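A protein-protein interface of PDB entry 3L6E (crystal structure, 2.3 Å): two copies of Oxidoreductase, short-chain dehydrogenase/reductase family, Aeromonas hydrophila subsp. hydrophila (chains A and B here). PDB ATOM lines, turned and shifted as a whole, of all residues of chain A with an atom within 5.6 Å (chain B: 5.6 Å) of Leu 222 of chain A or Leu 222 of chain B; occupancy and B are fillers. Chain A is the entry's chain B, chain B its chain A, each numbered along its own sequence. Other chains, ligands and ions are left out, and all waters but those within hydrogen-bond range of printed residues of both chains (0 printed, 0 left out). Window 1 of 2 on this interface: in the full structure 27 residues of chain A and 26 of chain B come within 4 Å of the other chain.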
ATOM      1  N   ASN A 175      13.280  31.203 -21.628  1.00  0.00           N
ATOM      2  CA  ASN A 175      13.230  31.059 -20.174  1.00  0.00           C
ATOM      3  C   ASN A 175      12.538  29.773 -19.799  1.00  0.00           C
ATOM      4  O   ASN A 175      11.475  29.482 -20.315  1.00  0.00           O
ATOM      5  CB  ASN A 175      12.505  32.236 -19.526  1.00  0.00           C
ATOM      6  CG  ASN A 175      13.298  33.520 -19.621  1.00  0.00           C
ATOM      7  OD1 ASN A 175      14.510  33.500 -19.820  1.00  0.00           O
ATOM      8  ND2 ASN A 175      12.616  34.650 -19.468  1.00  0.00           N
ATOM      9  N   LEU A 176      13.169  29.032 -18.898  1.00  0.00           N
ATOM     10  CA  LEU A 176      12.728  27.725 -18.467  1.00  0.00           C
ATOM     11  C   LEU A 176      12.559  27.703 -16.959  1.00  0.00           C
ATOM     12  O   LEU A 176      13.452  28.129 -16.231  1.00  0.00           O
ATOM     13  CB  LEU A 176      13.773  26.681 -18.857  1.00  0.00           C
ATOM     14  CG  LEU A 176      14.230  26.736 -20.323  1.00  0.00           C
ATOM     15  CD1 LEU A 176      15.470  25.873 -20.572  1.00  0.00           C
ATOM     16  CD2 LEU A 176      13.107  26.369 -21.262  1.00  0.00           C
ATOM     17  N   TYR A 177      11.409  27.189 -16.509  1.00  0.00           N
ATOM     18  CA  TYR A 177      11.016  27.261 -15.125  1.00  0.00           C
ATOM     19  C   TYR A 177      10.639  25.879 -14.577  1.00  0.00           C
ATOM     20  O   TYR A 177       9.461  25.496 -14.590  1.00  0.00           O
ATOM     21  CB  TYR A 177       9.822  28.195 -14.967  1.00  0.00           C
ATOM     22  CG  TYR A 177      10.041  29.622 -15.388  1.00  0.00           C
ATOM     23  CD1 TYR A 177       9.963  30.003 -16.741  1.00  0.00           C
ATOM     24  CD2 TYR A 177      10.274  30.610 -14.432  1.00  0.00           C
ATOM     25  CE1 TYR A 177      10.134  31.314 -17.113  1.00  0.00           C
ATOM     26  CE2 TYR A 177      10.456  31.927 -14.792  1.00  0.00           C
ATOM     27  CZ  TYR A 177      10.394  32.274 -16.135  1.00  0.00           C
ATOM     28  OH  TYR A 177      10.564  33.584 -16.478  1.00  0.00           O
ATOM     29  N   PRO A 178      11.631  25.124 -14.107  1.00  0.00           N
ATOM     30  CA  PRO A 178      11.352  23.873 -13.411  1.00  0.00           C
ATOM     31  C   PRO A 178      11.016  24.165 -11.954  1.00  0.00           C
ATOM     32  O   PRO A 178      11.907  24.453 -11.169  1.00  0.00           O
ATOM     33  CB  PRO A 178      12.678  23.113 -13.499  1.00  0.00           C
ATOM     34  CG  PRO A 178      13.718  24.116 -13.857  1.00  0.00           C
ATOM     35  CD  PRO A 178      13.069  25.440 -14.130  1.00  0.00           C
ATOM     36  N   TYR A 206      12.083  17.444 -20.840  1.00  0.00           N
ATOM     37  CA  TYR A 206      11.142  18.506 -21.234  1.00  0.00           C
ATOM     38  C   TYR A 206      11.836  19.761 -21.788  1.00  0.00           C
ATOM     39  O   TYR A 206      11.423  20.310 -22.821  1.00  0.00           O
ATOM     40  CB  TYR A 206      10.273  18.934 -20.048  1.00  0.00           C
ATOM     41  CG  TYR A 206       9.086  18.058 -19.774  1.00  0.00           C
ATOM     42  CD1 TYR A 206       8.168  17.752 -20.782  1.00  0.00           C
ATOM     43  CD2 TYR A 206       8.849  17.572 -18.490  1.00  0.00           C
ATOM     44  CE1 TYR A 206       7.074  16.944 -20.519  1.00  0.00           C
ATOM     45  CE2 TYR A 206       7.752  16.778 -18.219  1.00  0.00           C
ATOM     46  CZ  TYR A 206       6.868  16.474 -19.231  1.00  0.00           C
ATOM     47  OH  TYR A 206       5.780  15.687 -18.952  1.00  0.00           O
ATOM     48  N   MET A 207      12.893  20.195 -21.137  1.00  0.00           N
ATOM     49  CA  MET A 207      13.600  21.371 -21.558  1.00  0.00           C
ATOM     50  C   MET A 207      14.317  21.196 -22.878  1.00  0.00           C
ATOM     51  O   MET A 207      14.296  22.077 -23.697  1.00  0.00           O
ATOM     52  CB  MET A 207      14.571  21.798 -20.479  1.00  0.00           C
ATOM     53  CG  MET A 207      13.882  22.173 -19.208  1.00  0.00           C
ATOM     54  SD  MET A 207      15.081  22.306 -17.800  1.00  0.00           S
ATOM     55  CE  MET A 207      15.837  23.955 -18.179  1.00  0.00           C
ATOM     56  N   ALA A 210      11.908  21.107 -25.788  1.00  0.00           N
ATOM     57  CA  ALA A 210      11.439  22.462 -26.013  1.00  0.00           C
ATOM     58  C   ALA A 210      12.524  23.303 -26.679  1.00  0.00           C
ATOM     59  O   ALA A 210      12.234  24.269 -27.377  1.00  0.00           O
ATOM     60  CB  ALA A 210      11.016  23.093 -24.687  1.00  0.00           C
ATOM     61  N   VAL A 219      10.027  27.722 -28.828  1.00  0.00           N
ATOM     62  CA  VAL A 219       9.498  27.901 -27.485  1.00  0.00           C
ATOM     63  C   VAL A 219      10.236  29.036 -26.819  1.00  0.00           C
ATOM     64  O   VAL A 219      11.458  29.005 -26.762  1.00  0.00           O
ATOM     65  CB  VAL A 219       9.750  26.636 -26.605  1.00  0.00           C
ATOM     66  CG1 VAL A 219       9.277  26.882 -25.152  1.00  0.00           C
ATOM     67  CG2 VAL A 219       9.091  25.432 -27.205  1.00  0.00           C
ATOM     68  N   THR A 220       9.479  30.005 -26.291  1.00  0.00           N
ATOM     69  CA  THR A 220      10.012  31.192 -25.612  1.00  0.00           C
ATOM     70  C   THR A 220      10.052  31.010 -24.076  1.00  0.00           C
ATOM     71  O   THR A 220      10.977  31.506 -23.423  1.00  0.00           O
ATOM     72  CB  THR A 220       9.180  32.480 -25.952  1.00  0.00           C
ATOM     73  OG1 THR A 220       7.829  32.342 -25.478  1.00  0.00           O
ATOM     74  CG2 THR A 220       9.144  32.768 -27.444  1.00  0.00           C
ATOM     75  N   ASP A 221       9.052  30.303 -23.519  1.00  0.00           N
ATOM     76  CA  ASP A 221       8.945  30.064 -22.073  1.00  0.00           C
ATOM     77  C   ASP A 221       8.345  28.700 -21.714  1.00  0.00           C
ATOM     78  O   ASP A 221       7.258  28.344 -22.183  1.00  0.00           O
ATOM     79  CB  ASP A 221       8.089  31.154 -21.412  1.00  0.00           C
ATOM     80  CG  ASP A 221       8.476  32.537 -21.865  1.00  0.00           C
ATOM     81  OD1 ASP A 221       9.415  33.108 -21.286  1.00  0.00           O
ATOM     82  OD2 ASP A 221       7.849  33.028 -22.831  1.00  0.00           O
ATOM     83  N   LEU A 222       9.013  27.978 -20.816  1.00  0.00           N
ATOM     84  CA  LEU A 222       8.522  26.666 -20.404  1.00  0.00           C
ATOM     85  C   LEU A 222       8.345  26.599 -18.890  1.00  0.00           C
ATOM     86  O   LEU A 222       9.269  26.864 -18.135  1.00  0.00           O
ATOM     87  CB  LEU A 222       9.474  25.573 -20.878  1.00  0.00           C
ATOM     88  CG  LEU A 222       9.131  24.111 -20.590  1.00  0.00           C
ATOM     89  CD1 LEU A 222       8.012  23.667 -21.465  1.00  0.00           C
ATOM     90  CD2 LEU A 222      10.344  23.252 -20.871  1.00  0.00           C
ATOM     91  N   PHE A 223       7.144  26.259 -18.454  1.00  0.00           N
ATOM     92  CA  PHE A 223       6.884  26.138 -17.048  1.00  0.00           C
ATOM     93  C   PHE A 223       6.648  24.651 -16.749  1.00  0.00           C
ATOM     94  O   PHE A 223       5.761  24.040 -17.320  1.00  0.00           O
ATOM     95  CB  PHE A 223       5.696  27.002 -16.665  1.00  0.00           C
ATOM     96  CG  PHE A 223       5.960  28.480 -16.763  1.00  0.00           C
ATOM     97  CD1 PHE A 223       5.887  29.134 -17.982  1.00  0.00           C
ATOM     98  CD2 PHE A 223       6.234  29.231 -15.610  1.00  0.00           C
ATOM     99  CE1 PHE A 223       6.106  30.521 -18.067  1.00  0.00           C
ATOM    100  CE2 PHE A 223       6.447  30.601 -15.687  1.00  0.00           C
ATOM    101  CZ  PHE A 223       6.392  31.248 -16.921  1.00  0.00           C
ATOM    102  N   ILE A 224       7.508  24.066 -15.915  1.00  0.00           N
ATOM    103  CA  ILE A 224       7.359  22.675 -15.491  1.00  0.00           C
ATOM    104  C   ILE A 224       7.003  22.638 -14.014  1.00  0.00           C
ATOM    105  O   ILE A 224       7.612  23.339 -13.180  1.00  0.00           O
ATOM    106  CB  ILE A 224       8.614  21.832 -15.746  1.00  0.00           C
ATOM    107  CG1 ILE A 224       9.064  21.956 -17.206  1.00  0.00           C
ATOM    108  CG2 ILE A 224       8.347  20.341 -15.411  1.00  0.00           C
ATOM    109  CD1 ILE A 224      10.499  21.586 -17.416  1.00  0.00           C
ATOM    110  N   ASN B 175      -1.838  24.992 -20.057  1.00  0.00           N
ATOM    111  CA  ASN B 175      -2.207  26.102 -20.935  1.00  0.00           C
ATOM    112  C   ASN B 175      -1.121  26.322 -22.000  1.00  0.00           C
ATOM    113  O   ASN B 175       0.026  26.480 -21.668  1.00  0.00           O
ATOM    114  CB  ASN B 175      -2.433  27.365 -20.114  1.00  0.00           C
ATOM    115  CG  ASN B 175      -3.628  27.267 -19.187  1.00  0.00           C
ATOM    116  OD1 ASN B 175      -4.600  26.548 -19.445  1.00  0.00           O
ATOM    117  ND2 ASN B 175      -3.570  28.014 -18.100  1.00  0.00           N
ATOM    118  N   LEU B 176      -1.493  26.317 -23.272  1.00  0.00           N
ATOM    119  CA  LEU B 176      -0.519  26.369 -24.362  1.00  0.00           C
ATOM    120  C   LEU B 176      -0.748  27.631 -25.206  1.00  0.00           C
ATOM    121  O   LEU B 176      -1.874  27.908 -25.584  1.00  0.00           O
ATOM    122  CB  LEU B 176      -0.648  25.122 -25.252  1.00  0.00           C
ATOM    123  CG  LEU B 176      -0.721  23.763 -24.523  1.00  0.00           C
ATOM    124  CD1 LEU B 176      -1.310  22.683 -25.401  1.00  0.00           C
ATOM    125  CD2 LEU B 176       0.618  23.324 -23.978  1.00  0.00           C
ATOM    126  N   TYR B 177       0.336  28.356 -25.501  1.00  0.00           N
ATOM    127  CA  TYR B 177       0.272  29.657 -26.155  1.00  0.00           C
ATOM    128  C   TYR B 177       1.106  29.746 -27.445  1.00  0.00           C
ATOM    129  O   TYR B 177       2.251  30.189 -27.417  1.00  0.00           O
ATOM    130  CB  TYR B 177       0.735  30.737 -25.170  1.00  0.00           C
ATOM    131  CG  TYR B 177      -0.040  30.768 -23.873  1.00  0.00           C
ATOM    132  CD1 TYR B 177       0.205  29.817 -22.844  1.00  0.00           C
ATOM    133  CD2 TYR B 177      -0.993  31.752 -23.648  1.00  0.00           C
ATOM    134  CE1 TYR B 177      -0.496  29.873 -21.637  1.00  0.00           C
ATOM    135  CE2 TYR B 177      -1.698  31.823 -22.457  1.00  0.00           C
ATOM    136  CZ  TYR B 177      -1.445  30.889 -21.448  1.00  0.00           C
ATOM    137  OH  TYR B 177      -2.178  30.958 -20.279  1.00  0.00           O
ATOM    138  N   PRO B 178       0.564  29.274 -28.558  1.00  0.00           N
ATOM    139  CA  PRO B 178       1.214  29.500 -29.853  1.00  0.00           C
ATOM    140  C   PRO B 178       0.905  30.911 -30.317  1.00  0.00           C
ATOM    141  O   PRO B 178      -0.236  31.175 -30.661  1.00  0.00           O
ATOM    142  CB  PRO B 178       0.478  28.540 -30.801  1.00  0.00           C
ATOM    143  CG  PRO B 178      -0.570  27.834 -29.977  1.00  0.00           C
ATOM    144  CD  PRO B 178      -0.731  28.587 -28.698  1.00  0.00           C
ATOM    145  N   TYR B 206       5.832  20.863 -30.819  1.00  0.00           N
ATOM    146  CA  TYR B 206       6.207  21.380 -29.499  1.00  0.00           C
ATOM    147  C   TYR B 206       5.177  21.040 -28.437  1.00  0.00           C
ATOM    148  O   TYR B 206       5.536  20.637 -27.342  1.00  0.00           O
ATOM    149  CB  TYR B 206       6.364  22.906 -29.498  1.00  0.00           C
ATOM    150  CG  TYR B 206       7.667  23.392 -30.071  1.00  0.00           C
ATOM    151  CD1 TYR B 206       8.889  22.928 -29.574  1.00  0.00           C
ATOM    152  CD2 TYR B 206       7.681  24.303 -31.117  1.00  0.00           C
ATOM    153  CE1 TYR B 206      10.090  23.374 -30.119  1.00  0.00           C
ATOM    154  CE2 TYR B 206       8.859  24.754 -31.644  1.00  0.00           C
ATOM    155  CZ  TYR B 206      10.054  24.299 -31.141  1.00  0.00           C
ATOM    156  OH  TYR B 206      11.219  24.768 -31.703  1.00  0.00           O
ATOM    157  N   MET B 207       3.906  21.248 -28.777  1.00  0.00           N
ATOM    158  CA  MET B 207       2.787  21.067 -27.856  1.00  0.00           C
ATOM    159  C   MET B 207       2.656  19.593 -27.431  1.00  0.00           C
ATOM    160  O   MET B 207       2.525  19.297 -26.244  1.00  0.00           O
ATOM    161  CB  MET B 207       1.478  21.578 -28.479  1.00  0.00           C
ATOM    162  CG  MET B 207       1.443  23.086 -28.716  1.00  0.00           C
ATOM    163  SD  MET B 207      -0.127  23.729 -29.736  1.00  0.00           S
ATOM    164  CE  MET B 207      -1.438  23.718 -28.350  1.00  0.00           C
ATOM    165  N   ALA B 210       5.423  18.567 -25.299  1.00  0.00           N
ATOM    166  CA  ALA B 210       5.197  19.130 -23.988  1.00  0.00           C
ATOM    167  C   ALA B 210       4.125  18.316 -23.229  1.00  0.00           C
ATOM    168  O   ALA B 210       4.191  18.190 -22.026  1.00  0.00           O
ATOM    169  CB  ALA B 210       4.802  20.581 -24.104  1.00  0.00           C
ATOM    170  N   VAL B 219       4.482  19.594 -17.861  1.00  0.00           N
ATOM    171  CA  VAL B 219       4.508  20.992 -18.294  1.00  0.00           C
ATOM    172  C   VAL B 219       3.166  21.622 -17.932  1.00  0.00           C
ATOM    173  O   VAL B 219       2.127  21.068 -18.245  1.00  0.00           O
ATOM    174  CB  VAL B 219       4.738  21.069 -19.831  1.00  0.00           C
ATOM    175  CG1 VAL B 219       4.302  22.441 -20.405  1.00  0.00           C
ATOM    176  CG2 VAL B 219       6.171  20.765 -20.146  1.00  0.00           C
ATOM    177  N   THR B 220       3.191  22.775 -17.275  1.00  0.00           N
ATOM    178  CA  THR B 220       1.959  23.459 -16.898  1.00  0.00           C
ATOM    179  C   THR B 220       1.588  24.562 -17.893  1.00  0.00           C
ATOM    180  O   THR B 220       0.409  24.847 -18.092  1.00  0.00           O
ATOM    181  CB  THR B 220       2.047  24.053 -15.478  1.00  0.00           C
ATOM    182  OG1 THR B 220       3.196  24.900 -15.392  1.00  0.00           O
ATOM    183  CG2 THR B 220       2.137  22.924 -14.385  1.00  0.00           C
ATOM    184  N   ASP B 221       2.600  25.167 -18.517  1.00  0.00           N
ATOM    185  CA  ASP B 221       2.401  26.286 -19.445  1.00  0.00           C
ATOM    186  C   ASP B 221       3.469  26.277 -20.520  1.00  0.00           C
ATOM    187  O   ASP B 221       4.658  26.107 -20.235  1.00  0.00           O
ATOM    188  CB  ASP B 221       2.413  27.659 -18.718  1.00  0.00           C
ATOM    189  CG  ASP B 221       1.579  27.661 -17.437  1.00  0.00           C
ATOM    190  OD1 ASP B 221       0.377  28.050 -17.459  1.00  0.00           O
ATOM    191  OD2 ASP B 221       2.144  27.267 -16.396  1.00  0.00           O
ATOM    192  N   LEU B 222       3.043  26.484 -21.758  1.00  0.00           N
ATOM    193  CA  LEU B 222       3.969  26.476 -22.890  1.00  0.00           C
ATOM    194  C   LEU B 222       3.734  27.674 -23.820  1.00  0.00           C
ATOM    195  O   LEU B 222       2.676  27.808 -24.373  1.00  0.00           O
ATOM    196  CB  LEU B 222       3.823  25.175 -23.685  1.00  0.00           C
ATOM    197  CG  LEU B 222       4.740  24.984 -24.889  1.00  0.00           C
ATOM    198  CD1 LEU B 222       6.196  24.754 -24.471  1.00  0.00           C
ATOM    199  CD2 LEU B 222       4.249  23.867 -25.811  1.00  0.00           C
ATOM    200  N   PHE B 223       4.747  28.515 -23.993  1.00  0.00           N
ATOM    201  CA  PHE B 223       4.652  29.692 -24.845  1.00  0.00           C
ATOM    202  C   PHE B 223       5.522  29.483 -26.079  1.00  0.00           C
ATOM    203  O   PHE B 223       6.718  29.252 -25.967  1.00  0.00           O
ATOM    204  CB  PHE B 223       5.074  30.958 -24.075  1.00  0.00           C
ATOM    205  CG  PHE B 223       4.164  31.302 -22.925  1.00  0.00           C
ATOM    206  CD1 PHE B 223       4.258  30.622 -21.711  1.00  0.00           C
ATOM    207  CD2 PHE B 223       3.204  32.305 -23.055  1.00  0.00           C
ATOM    208  CE1 PHE B 223       3.415  30.936 -20.639  1.00  0.00           C
ATOM    209  CE2 PHE B 223       2.355  32.617 -22.007  1.00  0.00           C
ATOM    210  CZ  PHE B 223       2.464  31.936 -20.785  1.00  0.00           C
ATOM    211  N   ILE B 224       4.904  29.520 -27.253  1.00  0.00           N
ATOM    212  CA  ILE B 224       5.648  29.394 -28.514  1.00  0.00           C
ATOM    213  C   ILE B 224       5.554  30.695 -29.291  1.00  0.00           C
ATOM    214  O   ILE B 224       4.463  31.226 -29.461  1.00  0.00           O
ATOM    215  CB  ILE B 224       5.083  28.265 -29.401  1.00  0.00           C
ATOM    216  CG1 ILE B 224       4.953  26.959 -28.609  1.00  0.00           C
ATOM    217  CG2 ILE B 224       5.965  28.048 -30.640  1.00  0.00           C
ATOM    218  CD1 ILE B 224       3.952  26.022 -29.241  1.00  0.00           C
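The backbone carbonyl oxygen of Phe 223 of chain A lies within hydrogen-bond range of the backbone NH of Thr 220 of chain B (2.9 Å). O of Asp 221 of chain B lies within hydrogen-bond range of N of Phe 223 of chain A, at 3.1 Å. The backbone carbonyl oxygen (O) of Phe 223 of chain B is in hydrogen-bond range of the backbone NH (N) of Thr 220 of chain A (2.9 Å). The backbone NH (N) of Phe 223 of chain B is in hydrogen-bond range of the backbone carbonyl oxygen (O) of Asp 221 of chain A, at 3.1 Å.
The backbone carbonyl oxygen (O) of Asn 175 of chain B is in hydrogen-bond range of the backbone NH (N) of Leu 222 of chain B (3.0 Å). The backbone NH (N) of Tyr 177 of chain B sits at hydrogen-bond distance from the backbone carbonyl oxygen (O) of Leu 222 of chain B, 2.7 Å away. The side-chain carboxylate (OD2) of Asp 221 of chain B sits at hydrogen-bond distance from the side-chain hydroxyl (OG1) of Thr 220 of chain B (2.8 Å). N of Asn 175 of chain A sits at hydrogen-bond distance from O of Thr 220 of chain A. The backbone carbonyl oxygen of Leu 222 of chain A is in hydrogen-bond range of the backbone NH of Tyr 177 of chain A, at 2.7 Å. OG1 of Thr 220 of chain A lies within hydrogen-bond range of OD2 of Asp 221 of chain A.
Ala 210 of chain A touches Tyr 206 of chain B (O to CE1, 3.6 Å). CG2 of Val 219 of chain A touches CD1 of Tyr 206 of chain B (3.5 Å). CG1 of Val 219 of chain A touches CD1 of Leu 222 of chain B, at 3.8 Å. Phe 223 of chain B touches Val 219 of chain A (O to CA, 3.4 Å). Asp 221 of chain A touches Asp 221 of chain B (O to O, 3.9 Å). Val 219 of chain B touches Leu 222 of chain A. Leu 222 of chain A touches Asp 221 of chain B (CA to O, 3.9 Å). Leu 222 of chain B touches Leu 222 of chain A. CA of Val 219 of chain B touches O of Phe 223 of chain A, at 3.4 Å. Phe 223 of chain A touches Phe 223 of chain B (CE1 to CE1, 3.7 Å).
Printed residues of chain B within 4 Å of Tyr 206 of chain A: Ala 210 and Val 219. Printed residues of chain B within 4 Å of Ala 210 of chain A: Tyr 206. Of the printed residues of chain B, Asp 221 of chain A touches Asp 221 (3.9 Å), Leu 222 (3.8 Å) and Phe 223 (3.1 Å). Leu 222 of chain A touches three residues of chain B. Of the printed residues of chain B, Phe 223 of chain A touches Val 219 (3.4 Å), Thr 220 (2.9 Å), Asp 221 (3.1 Å) and Phe 223 (3.7 Å). Of the printed residues of chain A, Ala 210 of chain B touches Tyr 206. Of the printed residues of chain A, Leu 222 of chain B touches Val 219, Asp 221 and Leu 222. The nearest residue of chain A that does not touch Leu 222 of chain B is Ala 210 of chain A (5.1 Å).
Of the 13 printed residues of chain B, 7 touch a printed residue of chain A. Printed residues of chain B that touch a printed residue of chain A: Tyr 206, Ala 210, Val 219, Thr 220, Asp 221, Leu 222 and Phe 223. Along chain B the printed residues that touch a printed residue of chain A span positions 206 to 223. Among the printed residues, 17 pairs touch across the chains. Among the printed residues, no Asp or Glu carboxylate lies within 4 Å of a Lys or Arg side-chain nitrogen of the other chain.
Tyr 206 of chain A touches Ala 210 of chain B, and with the chains exchanged Ala 210 of chain A touches Tyr 206 of chain B. Tyr 206 of chain A touches Val 219 of chain B, and with the chains exchanged Val 219 of chain A touches Tyr 206 of chain B. Val 219 of chain A touches Leu 222 of chain B, and with the chains exchanged Leu 222 of chain A touches Val 219 of chain B. Phe 223 of chain A touches its own counterpart, Phe 223 of chain B.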
